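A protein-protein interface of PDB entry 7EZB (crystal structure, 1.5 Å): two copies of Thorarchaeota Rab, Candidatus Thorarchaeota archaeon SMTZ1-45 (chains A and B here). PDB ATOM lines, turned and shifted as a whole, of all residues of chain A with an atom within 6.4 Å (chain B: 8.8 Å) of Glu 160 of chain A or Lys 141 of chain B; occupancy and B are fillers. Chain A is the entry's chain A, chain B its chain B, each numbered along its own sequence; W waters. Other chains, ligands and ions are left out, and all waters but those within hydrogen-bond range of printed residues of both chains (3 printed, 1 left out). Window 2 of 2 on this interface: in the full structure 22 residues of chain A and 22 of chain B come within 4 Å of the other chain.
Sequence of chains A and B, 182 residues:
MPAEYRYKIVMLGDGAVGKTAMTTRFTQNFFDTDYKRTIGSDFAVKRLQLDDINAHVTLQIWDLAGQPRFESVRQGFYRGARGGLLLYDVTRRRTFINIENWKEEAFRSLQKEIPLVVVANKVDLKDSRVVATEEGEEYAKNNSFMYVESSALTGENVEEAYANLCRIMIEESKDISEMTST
O of Glu 138 of chain B sits close to ND2 of Asn 142 of chain B (3.3 Å). The side-chain carboxylate (OE1) of Glu 160 of chain A sits close to the side-chain amide oxygen (OD1) of Asn 164 of chain A.
1 position is printed for both chains. Of the 7 pairs that touch across the chains among the printed residues, none has its exchanged pair printed and touching as well.
Glu 160 of chain A touches just one residue of chain B: Lys 141. Printed residues of chain A within 4 Å of Lys 141 of chain B: Met 146 (3.5 Å), Glu 160 (3.8 Å), Asn 164 (3.2 Å) and Ile 168 (3.6 Å). No residue of chain B comes within 4 Å of Ala 161 of chain A. Printed residues of chain B within 4 Å of Asn 164 of chain A: Lys 141 (3.2 Å). Of the printed residues of chain A, Asn 142 of chain B touches Arg 167 (3.5 Å) and Ile 168 (3.4 Å). Of the printed residues of chain B, Ile 168 of chain A touches Lys 141, Asn 142 and Ser 144. Of the printed residues of chain B, Met 146 of chain A touches Lys 141 (3.5 Å). Of the printed residues of chain A, Ser 144 of chain B touches Ile 168. The nearest printed residue of chain B that does not touch Glu 160 of chain A is Asn 142 of chain B (7.9 Å). The nearest printed residue of chain A that does not touch Lys 141 of chain B is Arg 167 of chain A (5.7 Å).
Among the printed residues, pairs that only touch across the chains: Ile 168 of chain A with Asn 142 of chain B, Arg 167 of chain A with Asn 142 of chain B, Met 146 of chain A with Lys 141 of chain B, Ile 168 of chain A with Lys 141 of chain B and Ile 168 of chain A with Ser 144 of chain B.
Printed residues of chain B that touch a printed residue of chain A: Lys 141, Asn 142 and Ser 144. Of the 14 printed residues of chain A, 5 touch a printed residue of chain B. Printed residues of chain A that touch a printed residue of chain B: Met 146, Glu 160, Asn 164, Arg 167 and Ile 168. Hydrophobic or aromatic side chains of chain A within 4 Å of the printed part of chain B: Met 146 and Ile 168. Along chain A the printed residues that touch a printed residue of chain B span positions 146 to 168. Among the printed residues, 7 pairs touch across the chains. Among the printed residues, Asp or Glu carboxylates within 4 Å of a Lys or Arg side-chain nitrogen of the other chain: Glu 160 of chain A with Lys 141 of chain B.
Water W3 bridges OD1 of Asn 164 of chain A and NZ of Lys 141 of chain B. Water W1 bridges the backbone carbonyl oxygen of Phe 145 of chain B (2.8 Å) and the side-chain sulfur of Met 146 of chain A (3.6 Å). Water W2 bridges N of Met 146 of chain A (2.8 Å) and OG of Ser 144 of chain B (2.9 Å).
The side-chain amino group (NZ) of Lys 141 of chain B is in salt-bridge range of the side-chain carboxylate (OE1) of Glu 160 of chain A (3.8 Å). OD1 of Asn 164 of chain A is in hydrogen-bond range of NZ of Lys 141 of chain B, at 3.2 Å.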
ATOM      1  N   PHE A  26      -2.592  39.180  14.519  1.00  0.00           N
ATOM      2  CA  PHE A  26      -1.173  39.285  14.185  1.00  0.00           C
ATOM      3  C   PHE A  26      -0.904  40.377  13.154  1.00  0.00           C
ATOM      4  O   PHE A  26       0.088  41.111  13.259  1.00  0.00           O
ATOM      5  CB  PHE A  26      -0.722  37.929  13.664  1.00  0.00           C
ATOM      6  CG  PHE A  26       0.740  37.825  13.357  1.00  0.00           C
ATOM      7  CD1 PHE A  26       1.710  38.204  14.275  1.00  0.00           C
ATOM      8  CD2 PHE A  26       1.135  37.245  12.163  1.00  0.00           C
ATOM      9  CE1 PHE A  26       3.074  38.045  13.982  1.00  0.00           C
ATOM     10  CE2 PHE A  26       2.487  37.078  11.862  1.00  0.00           C
ATOM     11  CZ  PHE A  26       3.450  37.480  12.768  1.00  0.00           C
ATOM     12  N   MET A 146       6.372  22.685  19.074  1.00  0.00           N
ATOM     13  CA  MET A 146       6.215  23.622  20.173  1.00  0.00           C
ATOM     14  C   MET A 146       4.729  23.819  20.487  1.00  0.00           C
ATOM     15  O   MET A 146       3.847  23.499  19.693  1.00  0.00           O
ATOM     16  CB  MET A 146       6.925  24.945  19.861  1.00  0.00           C
ATOM     17  CG  MET A 146       8.414  24.783  19.475  1.00  0.00           C
ATOM     18  SD  MET A 146       9.496  23.978  20.697  1.00  0.00           S
ATOM     19  CE  MET A 146       9.294  25.049  22.116  1.00  0.00           C
ATOM     20  N   VAL A 148       1.873  26.568  22.355  1.00  0.00           N
ATOM     21  CA  VAL A 148       1.606  27.940  22.790  1.00  0.00           C
ATOM     22  C   VAL A 148       0.145  28.042  23.202  1.00  0.00           C
ATOM     23  O   VAL A 148      -0.737  27.580  22.475  1.00  0.00           O
ATOM     24  CB  VAL A 148       1.901  28.937  21.654  1.00  0.00           C
ATOM     25  CG1 VAL A 148       1.517  30.364  22.086  1.00  0.00           C
ATOM     26  CG2 VAL A 148       3.387  28.900  21.260  1.00  0.00           C
ATOM     27  N   ASN A 157       0.260  35.946  23.622  1.00  0.00           N
ATOM     28  CA  ASN A 157       1.147  35.003  22.943  1.00  0.00           C
ATOM     29  C   ASN A 157       0.898  34.854  21.446  1.00  0.00           C
ATOM     30  O   ASN A 157       1.444  33.934  20.832  1.00  0.00           O
ATOM     31  CB  ASN A 157       1.157  33.620  23.610  1.00  0.00           C
ATOM     32  CG  ASN A 157       1.677  33.665  25.020  1.00  0.00           C
ATOM     33  OD1 ASN A 157       2.509  34.515  25.369  1.00  0.00           O
ATOM     34  ND2 ASN A 157       1.193  32.757  25.852  1.00  0.00           N
ATOM     35  N   VAL A 158       0.106  35.718  20.823  1.00  0.00           N
ATOM     36  CA  VAL A 158      -0.163  35.548  19.398  1.00  0.00           C
ATOM     37  C   VAL A 158       1.091  35.810  18.573  1.00  0.00           C
ATOM     38  O   VAL A 158       1.489  34.984  17.743  1.00  0.00           O
ATOM     39  CB  VAL A 158      -1.345  36.429  18.960  1.00  0.00           C
ATOM     40  CG1 VAL A 158      -1.477  36.456  17.411  1.00  0.00           C
ATOM     41  CG2 VAL A 158      -2.615  35.897  19.618  1.00  0.00           C
ATOM     42  N   GLU A 159       1.726  36.962  18.773  1.00  0.00           N
ATOM     43  CA  GLU A 159       2.980  37.220  18.064  1.00  0.00           C
ATOM     44  C   GLU A 159       4.015  36.149  18.387  1.00  0.00           C
ATOM     45  O   GLU A 159       4.758  35.704  17.503  1.00  0.00           O
ATOM     46  CB  GLU A 159       3.490  38.614  18.438  1.00  0.00           C
ATOM     47  CG  GLU A 159       4.582  39.164  17.521  1.00  0.00           C
ATOM     48  CD  GLU A 159       5.966  38.770  17.977  1.00  0.00           C
ATOM     49  OE1 GLU A 159       6.080  38.207  19.087  1.00  0.00           O
ATOM     50  OE2 GLU A 159       6.938  39.024  17.231  1.00  0.00           O
ATOM     51  N   GLU A 160       4.055  35.701  19.644  1.00  0.00           N
ATOM     52  CA  GLU A 160       5.012  34.688  20.055  1.00  0.00           C
ATOM     53  C   GLU A 160       4.856  33.417  19.229  1.00  0.00           C
ATOM     54  O   GLU A 160       5.852  32.821  18.805  1.00  0.00           O
ATOM     55  CB  GLU A 160       4.833  34.377  21.541  1.00  0.00           C
ATOM     56  CG  GLU A 160       5.812  33.357  22.084  1.00  0.00           C
ATOM     57  CD  GLU A 160       7.228  33.905  22.169  1.00  0.00           C
ATOM     58  OE1 GLU A 160       8.184  33.099  22.175  1.00  0.00           O
ATOM     59  OE2 GLU A 160       7.385  35.145  22.230  1.00  0.00           O
ATOM     60  N   ALA A 161       3.614  32.977  18.992  1.00  0.00           N
ATOM     61  CA  ALA A 161       3.419  31.755  18.217  1.00  0.00           C
ATOM     62  C   ALA A 161       3.974  31.904  16.805  1.00  0.00           C
ATOM     63  O   ALA A 161       4.676  31.014  16.302  1.00  0.00           O
ATOM     64  CB  ALA A 161       1.929  31.385  18.166  1.00  0.00           C
ATOM     65  N   TYR A 162       3.652  33.010  16.138  1.00  0.00           N
ATOM     66  CA  TYR A 162       4.165  33.201  14.784  1.00  0.00           C
ATOM     67  C   TYR A 162       5.675  33.387  14.782  1.00  0.00           C
ATOM     68  O   TYR A 162       6.362  32.865  13.890  1.00  0.00           O
ATOM     69  CB  TYR A 162       3.490  34.395  14.112  1.00  0.00           C
ATOM     70  CG  TYR A 162       2.041  34.189  13.703  1.00  0.00           C
ATOM     71  CD1 TYR A 162       1.011  34.643  14.519  1.00  0.00           C
ATOM     72  CD2 TYR A 162       1.707  33.648  12.463  1.00  0.00           C
ATOM     73  CE1 TYR A 162      -0.312  34.502  14.139  1.00  0.00           C
ATOM     74  CE2 TYR A 162       0.372  33.507  12.072  1.00  0.00           C
ATOM     75  CZ  TYR A 162      -0.631  33.955  12.918  1.00  0.00           C
ATOM     76  OH  TYR A 162      -1.960  33.854  12.571  1.00  0.00           O
ATOM     77  N   ALA A 163       6.214  34.121  15.764  1.00  0.00           N
ATOM     78  CA  ALA A 163       7.658  34.334  15.814  1.00  0.00           C
ATOM     79  C   ALA A 163       8.395  33.021  16.034  1.00  0.00           C
ATOM     80  O   ALA A 163       9.463  32.797  15.445  1.00  0.00           O
ATOM     81  CB  ALA A 163       7.994  35.363  16.905  1.00  0.00           C
ATOM     82  N   ASN A 164       7.861  32.157  16.900  1.00  0.00           N
ATOM     83  CA  ASN A 164       8.466  30.844  17.119  1.00  0.00           C
ATOM     84  C   ASN A 164       8.525  30.072  15.811  1.00  0.00           C
ATOM     85  O   ASN A 164       9.541  29.462  15.466  1.00  0.00           O
ATOM     86  CB  ASN A 164       7.649  30.054  18.145  1.00  0.00           C
ATOM     87  CG  ASN A 164       7.722  30.638  19.559  1.00  0.00           C
ATOM     88  OD1 ASN A 164       8.629  31.401  19.900  1.00  0.00           O
ATOM     89  ND2 ASN A 164       6.757  30.260  20.389  1.00  0.00           N
ATOM     90  N   LEU A 165       7.414  30.070  15.069  1.00  0.00           N
ATOM     91  CA  LEU A 165       7.409  29.343  13.805  1.00  0.00           C
ATOM     92  C   LEU A 165       8.426  29.937  12.834  1.00  0.00           C
ATOM     93  O   LEU A 165       9.152  29.198  12.146  1.00  0.00           O
ATOM     94  CB  LEU A 165       6.006  29.380  13.212  1.00  0.00           C
ATOM     95  CG  LEU A 165       5.810  28.654  11.883  1.00  0.00           C
ATOM     96  CD1 LEU A 165       6.075  27.164  12.028  1.00  0.00           C
ATOM     97  CD2 LEU A 165       4.401  28.902  11.335  1.00  0.00           C
ATOM     98  N   ARG A 167      11.232  31.453  13.506  1.00  0.00           N
ATOM     99  CA  ARG A 167      12.596  31.066  13.855  1.00  0.00           C
ATOM    100  C   ARG A 167      12.875  29.629  13.432  1.00  0.00           C
ATOM    101  O   ARG A 167      13.965  29.324  12.925  1.00  0.00           O
ATOM    102  CB  ARG A 167      12.851  31.246  15.349  1.00  0.00           C
ATOM    103  CG  ARG A 167      14.296  30.955  15.743  1.00  0.00           C
ATOM    104  CD  ARG A 167      15.270  31.792  14.915  1.00  0.00           C
ATOM    105  NE  ARG A 167      16.671  31.481  15.200  1.00  0.00           N
ATOM    106  CZ  ARG A 167      17.359  32.000  16.213  1.00  0.00           C
ATOM    107  NH1 ARG A 167      16.767  32.846  17.048  1.00  0.00           N
ATOM    108  NH2 ARG A 167      18.644  31.673  16.393  1.00  0.00           N
ATOM    109  N   ILE A 168      11.899  28.736  13.615  1.00  0.00           N
ATOM    110  CA  ILE A 168      12.079  27.350  13.201  1.00  0.00           C
ATOM    111  C   ILE A 168      12.304  27.263  11.701  1.00  0.00           C
ATOM    112  O   ILE A 168      13.179  26.519  11.232  1.00  0.00           O
ATOM    113  CB  ILE A 168      10.881  26.497  13.656  1.00  0.00           C
ATOM    114  CG1 ILE A 168      10.853  26.456  15.187  1.00  0.00           C
ATOM    115  CG2 ILE A 168      10.948  25.089  13.045  1.00  0.00           C
ATOM    116  CD1 ILE A 168       9.490  26.025  15.750  1.00  0.00           C
ATOM    117  N   VAL B 118      17.484  17.776  22.693  1.00  0.00           N
ATOM    118  CA  VAL B 118      18.610  18.469  23.311  1.00  0.00           C
ATOM    119  C   VAL B 118      18.684  18.048  24.771  1.00  0.00           C
ATOM    120  O   VAL B 118      17.695  18.157  25.509  1.00  0.00           O
ATOM    121  CB  VAL B 118      18.437  19.991  23.185  1.00  0.00           C
ATOM    122  CG1 VAL B 118      19.530  20.736  23.975  1.00  0.00           C
ATOM    123  CG2 VAL B 118      18.422  20.409  21.710  1.00  0.00           C
ATOM    124  N   GLU B 134      17.453  28.329  30.734  1.00  0.00           N
ATOM    125  CA  GLU B 134      16.806  29.109  29.681  1.00  0.00           C
ATOM    126  C   GLU B 134      17.609  29.096  28.388  1.00  0.00           C
ATOM    127  O   GLU B 134      17.025  29.132  27.302  1.00  0.00           O
ATOM    128  CB  GLU B 134      16.579  30.554  30.131  1.00  0.00           C
ATOM    129  CG  GLU B 134      16.173  30.726  31.582  1.00  0.00           C
ATOM    130  CD  GLU B 134      17.366  30.708  32.516  1.00  0.00           C
ATOM    131  OE1 GLU B 134      18.180  31.660  32.478  1.00  0.00           O
ATOM    132  OE2 GLU B 134      17.500  29.730  33.275  1.00  0.00           O
ATOM    133  N   GLU B 135      18.941  29.040  28.479  1.00  0.00           N
ATOM    134  CA  GLU B 135      19.755  29.038  27.267  1.00  0.00           C
ATOM    135  C   GLU B 135      19.505  27.783  26.445  1.00  0.00           C
ATOM    136  O   GLU B 135      19.357  27.849  25.217  1.00  0.00           O
ATOM    137  CB  GLU B 135      21.232  29.124  27.629  1.00  0.00           C
ATOM    138  CG  GLU B 135      21.608  30.379  28.352  1.00  0.00           C
ATOM    139  CD  GLU B 135      23.095  30.457  28.559  1.00  0.00           C
ATOM    140  OE1 GLU B 135      23.551  30.182  29.689  1.00  0.00           O
ATOM    141  OE2 GLU B 135      23.803  30.771  27.580  1.00  0.00           O
ATOM    142  N   GLY B 136      19.484  26.623  27.107  1.00  0.00           N
ATOM    143  CA  GLY B 136      19.212  25.385  26.402  1.00  0.00           C
ATOM    144  C   GLY B 136      17.792  25.326  25.869  1.00  0.00           C
ATOM    145  O   GLY B 136      17.563  24.874  24.743  1.00  0.00           O
ATOM    146  N   GLU B 137      16.819  25.773  26.670  1.00  0.00           N
ATOM    147  CA  GLU B 137      15.435  25.789  26.209  1.00  0.00           C
ATOM    148  C   GLU B 137      15.295  26.634  24.955  1.00  0.00           C
ATOM    149  O   GLU B 137      14.536  26.277  24.041  1.00  0.00           O
ATOM    150  CB  GLU B 137      14.521  26.335  27.306  1.00  0.00           C
ATOM    151  CG  GLU B 137      14.391  25.407  28.497  1.00  0.00           C
ATOM    152  CD  GLU B 137      13.509  25.982  29.588  1.00  0.00           C
ATOM    153  OE1 GLU B 137      13.431  27.224  29.701  1.00  0.00           O
ATOM    154  OE2 GLU B 137      12.894  25.188  30.332  1.00  0.00           O
ATOM    155  N   GLU B 138      16.002  27.769  24.906  1.00  0.00           N
ATOM    156  CA  GLU B 138      15.919  28.660  23.750  1.00  0.00           C
ATOM    157  C   GLU B 138      16.498  28.000  22.506  1.00  0.00           C
ATOM    158  O   GLU B 138      15.884  28.024  21.431  1.00  0.00           O
ATOM    159  CB  GLU B 138      16.651  29.963  24.066  1.00  0.00           C
ATOM    160  CG  GLU B 138      16.812  30.911  22.896  1.00  0.00           C
ATOM    161  CD  GLU B 138      17.617  32.138  23.282  1.00  0.00           C
ATOM    162  OE1 GLU B 138      18.861  32.101  23.161  1.00  0.00           O
ATOM    163  OE2 GLU B 138      17.008  33.128  23.735  1.00  0.00           O
ATOM    164  N   TYR B 139      17.691  27.408  22.631  1.00  0.00           N
ATOM    165  CA  TYR B 139      18.283  26.717  21.489  1.00  0.00           C
ATOM    166  C   TYR B 139      17.341  25.648  20.957  1.00  0.00           C
ATOM    167  O   TYR B 139      17.128  25.529  19.739  1.00  0.00           O
ATOM    168  CB  TYR B 139      19.636  26.091  21.860  1.00  0.00           C
ATOM    169  CG  TYR B 139      20.201  25.322  20.683  1.00  0.00           C
ATOM    170  CD1 TYR B 139      20.888  25.976  19.676  1.00  0.00           C
ATOM    171  CD2 TYR B 139      19.982  23.953  20.549  1.00  0.00           C
ATOM    172  CE1 TYR B 139      21.377  25.284  18.572  1.00  0.00           C
ATOM    173  CE2 TYR B 139      20.473  23.260  19.454  1.00  0.00           C
ATOM    174  CZ  TYR B 139      21.162  23.930  18.474  1.00  0.00           C
ATOM    175  OH  TYR B 139      21.632  23.244  17.365  1.00  0.00           O
ATOM    176  N   ALA B 140      16.787  24.839  21.858  1.00  0.00           N
ATOM    177  CA  ALA B 140      15.896  23.762  21.432  1.00  0.00           C
ATOM    178  C   ALA B 140      14.659  24.321  20.735  1.00  0.00           C
ATOM    179  O   ALA B 140      14.290  23.859  19.645  1.00  0.00           O
ATOM    180  CB  ALA B 140      15.514  22.904  22.643  1.00  0.00           C
ATOM    181  N   LYS B 141      14.038  25.342  21.324  1.00  0.00           N
ATOM    182  CA  LYS B 141      12.826  25.931  20.755  1.00  0.00           C
ATOM    183  C   LYS B 141      13.067  26.475  19.353  1.00  0.00           C
ATOM    184  O   LYS B 141      12.191  26.370  18.484  1.00  0.00           O
ATOM    185  CB  LYS B 141      12.293  27.018  21.697  1.00  0.00           C
ATOM    186  CG  LYS B 141      11.153  27.863  21.143  1.00  0.00           C
ATOM    187  CD  LYS B 141      10.528  28.728  22.240  1.00  0.00           C
ATOM    188  CE  LYS B 141      11.418  29.903  22.617  1.00  0.00           C
ATOM    189  NZ  LYS B 141      11.356  31.008  21.620  1.00  0.00           N
ATOM    190  N   ASN B 142      14.232  27.086  19.122  1.00  0.00           N
ATOM    191  CA  ASN B 142      14.552  27.660  17.813  1.00  0.00           C
ATOM    192  C   ASN B 142      14.630  26.600  16.723  1.00  0.00           C
ATOM    193  O   ASN B 142      14.515  26.943  15.535  1.00  0.00           O
ATOM    194  CB  ASN B 142      15.911  28.373  17.879  1.00  0.00           C
ATOM    195  CG  ASN B 142      15.905  29.613  18.768  1.00  0.00           C
ATOM    196  OD1 ASN B 142      14.859  30.194  19.078  1.00  0.00           O
ATOM    197  ND2 ASN B 142      17.100  30.051  19.146  1.00  0.00           N
ATOM    198  N   ASN B 143      14.855  25.334  17.085  1.00  0.00           N
ATOM    199  CA  ASN B 143      14.962  24.239  16.123  1.00  0.00           C
ATOM    200  C   ASN B 143      13.774  23.286  16.198  1.00  0.00           C
ATOM    201  O   ASN B 143      13.794  22.231  15.548  1.00  0.00           O
ATOM    202  CB  ASN B 143      16.249  23.446  16.388  1.00  0.00           C
ATOM    203  CG  ASN B 143      17.482  24.193  15.954  1.00  0.00           C
ATOM    204  OD1 ASN B 143      17.867  24.137  14.783  1.00  0.00           O
ATOM    205  ND2 ASN B 143      18.105  24.926  16.880  1.00  0.00           N
ATOM    206  N   SER B 144      12.768  23.609  17.014  1.00  0.00           N
ATOM    207  CA  SER B 144      11.650  22.704  17.287  1.00  0.00           C
ATOM    208  C   SER B 144      12.117  21.362  17.851  1.00  0.00           C
ATOM    209  O   SER B 144      11.539  20.316  17.557  1.00  0.00           O
ATOM    210  CB  SER B 144      10.741  22.520  16.073  1.00  0.00           C
ATOM    211  OG  SER B 144       9.483  21.991  16.466  1.00  0.00           O
ATOM    212  N   PHE B 145      13.157  21.390  18.695  1.00  0.00           N
ATOM    213  CA  PHE B 145      13.644  20.220  19.419  1.00  0.00           C
ATOM    214  C   PHE B 145      13.072  20.242  20.831  1.00  0.00           C
ATOM    215  O   PHE B 145      12.858  21.316  21.425  1.00  0.00           O
ATOM    216  CB  PHE B 145      15.172  20.234  19.574  1.00  0.00           C
ATOM    217  CG  PHE B 145      15.958  20.122  18.284  1.00  0.00           C
ATOM    218  CD1 PHE B 145      15.441  19.475  17.166  1.00  0.00           C
ATOM    219  CD2 PHE B 145      17.248  20.639  18.214  1.00  0.00           C
ATOM    220  CE1 PHE B 145      16.210  19.372  15.986  1.00  0.00           C
ATOM    221  CE2 PHE B 145      18.024  20.528  17.058  1.00  0.00           C
ATOM    222  CZ  PHE B 145      17.503  19.896  15.941  1.00  0.00           C
ATOM    223  N   MET B 146      12.843  19.056  21.377  1.00  0.00           N
ATOM    224  CA  MET B 146      12.550  18.973  22.799  1.00  0.00           C
ATOM    225  C   MET B 146      13.831  19.155  23.614  1.00  0.00           C
ATOM    226  O   MET B 146      14.941  18.984  23.113  1.00  0.00           O
ATOM    227  CB  MET B 146      11.835  17.653  23.136  1.00  0.00           C
ATOM    228  CG  MET B 146      10.578  17.408  22.294  1.00  0.00           C
ATOM    229  SD  MET B 146       9.245  18.627  22.455  1.00  0.00           S
ATOM    230  CE  MET B 146       9.578  19.803  21.135  1.00  0.00           C
ATOM    231  N   TYR B 147      13.662  19.518  24.883  1.00  0.00           N
ATOM    232  CA  TYR B 147      14.776  19.831  25.771  1.00  0.00           C
ATOM    233  C   TYR B 147      14.581  19.115  27.103  1.00  0.00           C
ATOM    234  O   TYR B 147      13.493  19.168  27.694  1.00  0.00           O
ATOM    235  CB  TYR B 147      14.845  21.348  26.012  1.00  0.00           C
ATOM    236  CG  TYR B 147      15.850  21.756  27.060  1.00  0.00           C
ATOM    237  CD1 TYR B 147      17.198  21.870  26.751  1.00  0.00           C
ATOM    238  CD2 TYR B 147      15.442  22.043  28.361  1.00  0.00           C
ATOM    239  CE1 TYR B 147      18.124  22.249  27.714  1.00  0.00           C
ATOM    240  CE2 TYR B 147      16.353  22.420  29.326  1.00  0.00           C
ATOM    241  CZ  TYR B 147      17.692  22.529  28.992  1.00  0.00           C
ATOM    242  OH  TYR B 147      18.614  22.925  29.954  1.00  0.00           O
HETATM  243  O   HOH W   1      11.471  22.611  23.423  1.00  0.00           O
HETATM  244  O   HOH W   2       7.026  23.452  16.427  1.00  0.00           O
HETATM  245  O   HOH W   3      10.750  32.911  19.004  1.00  0.00           O
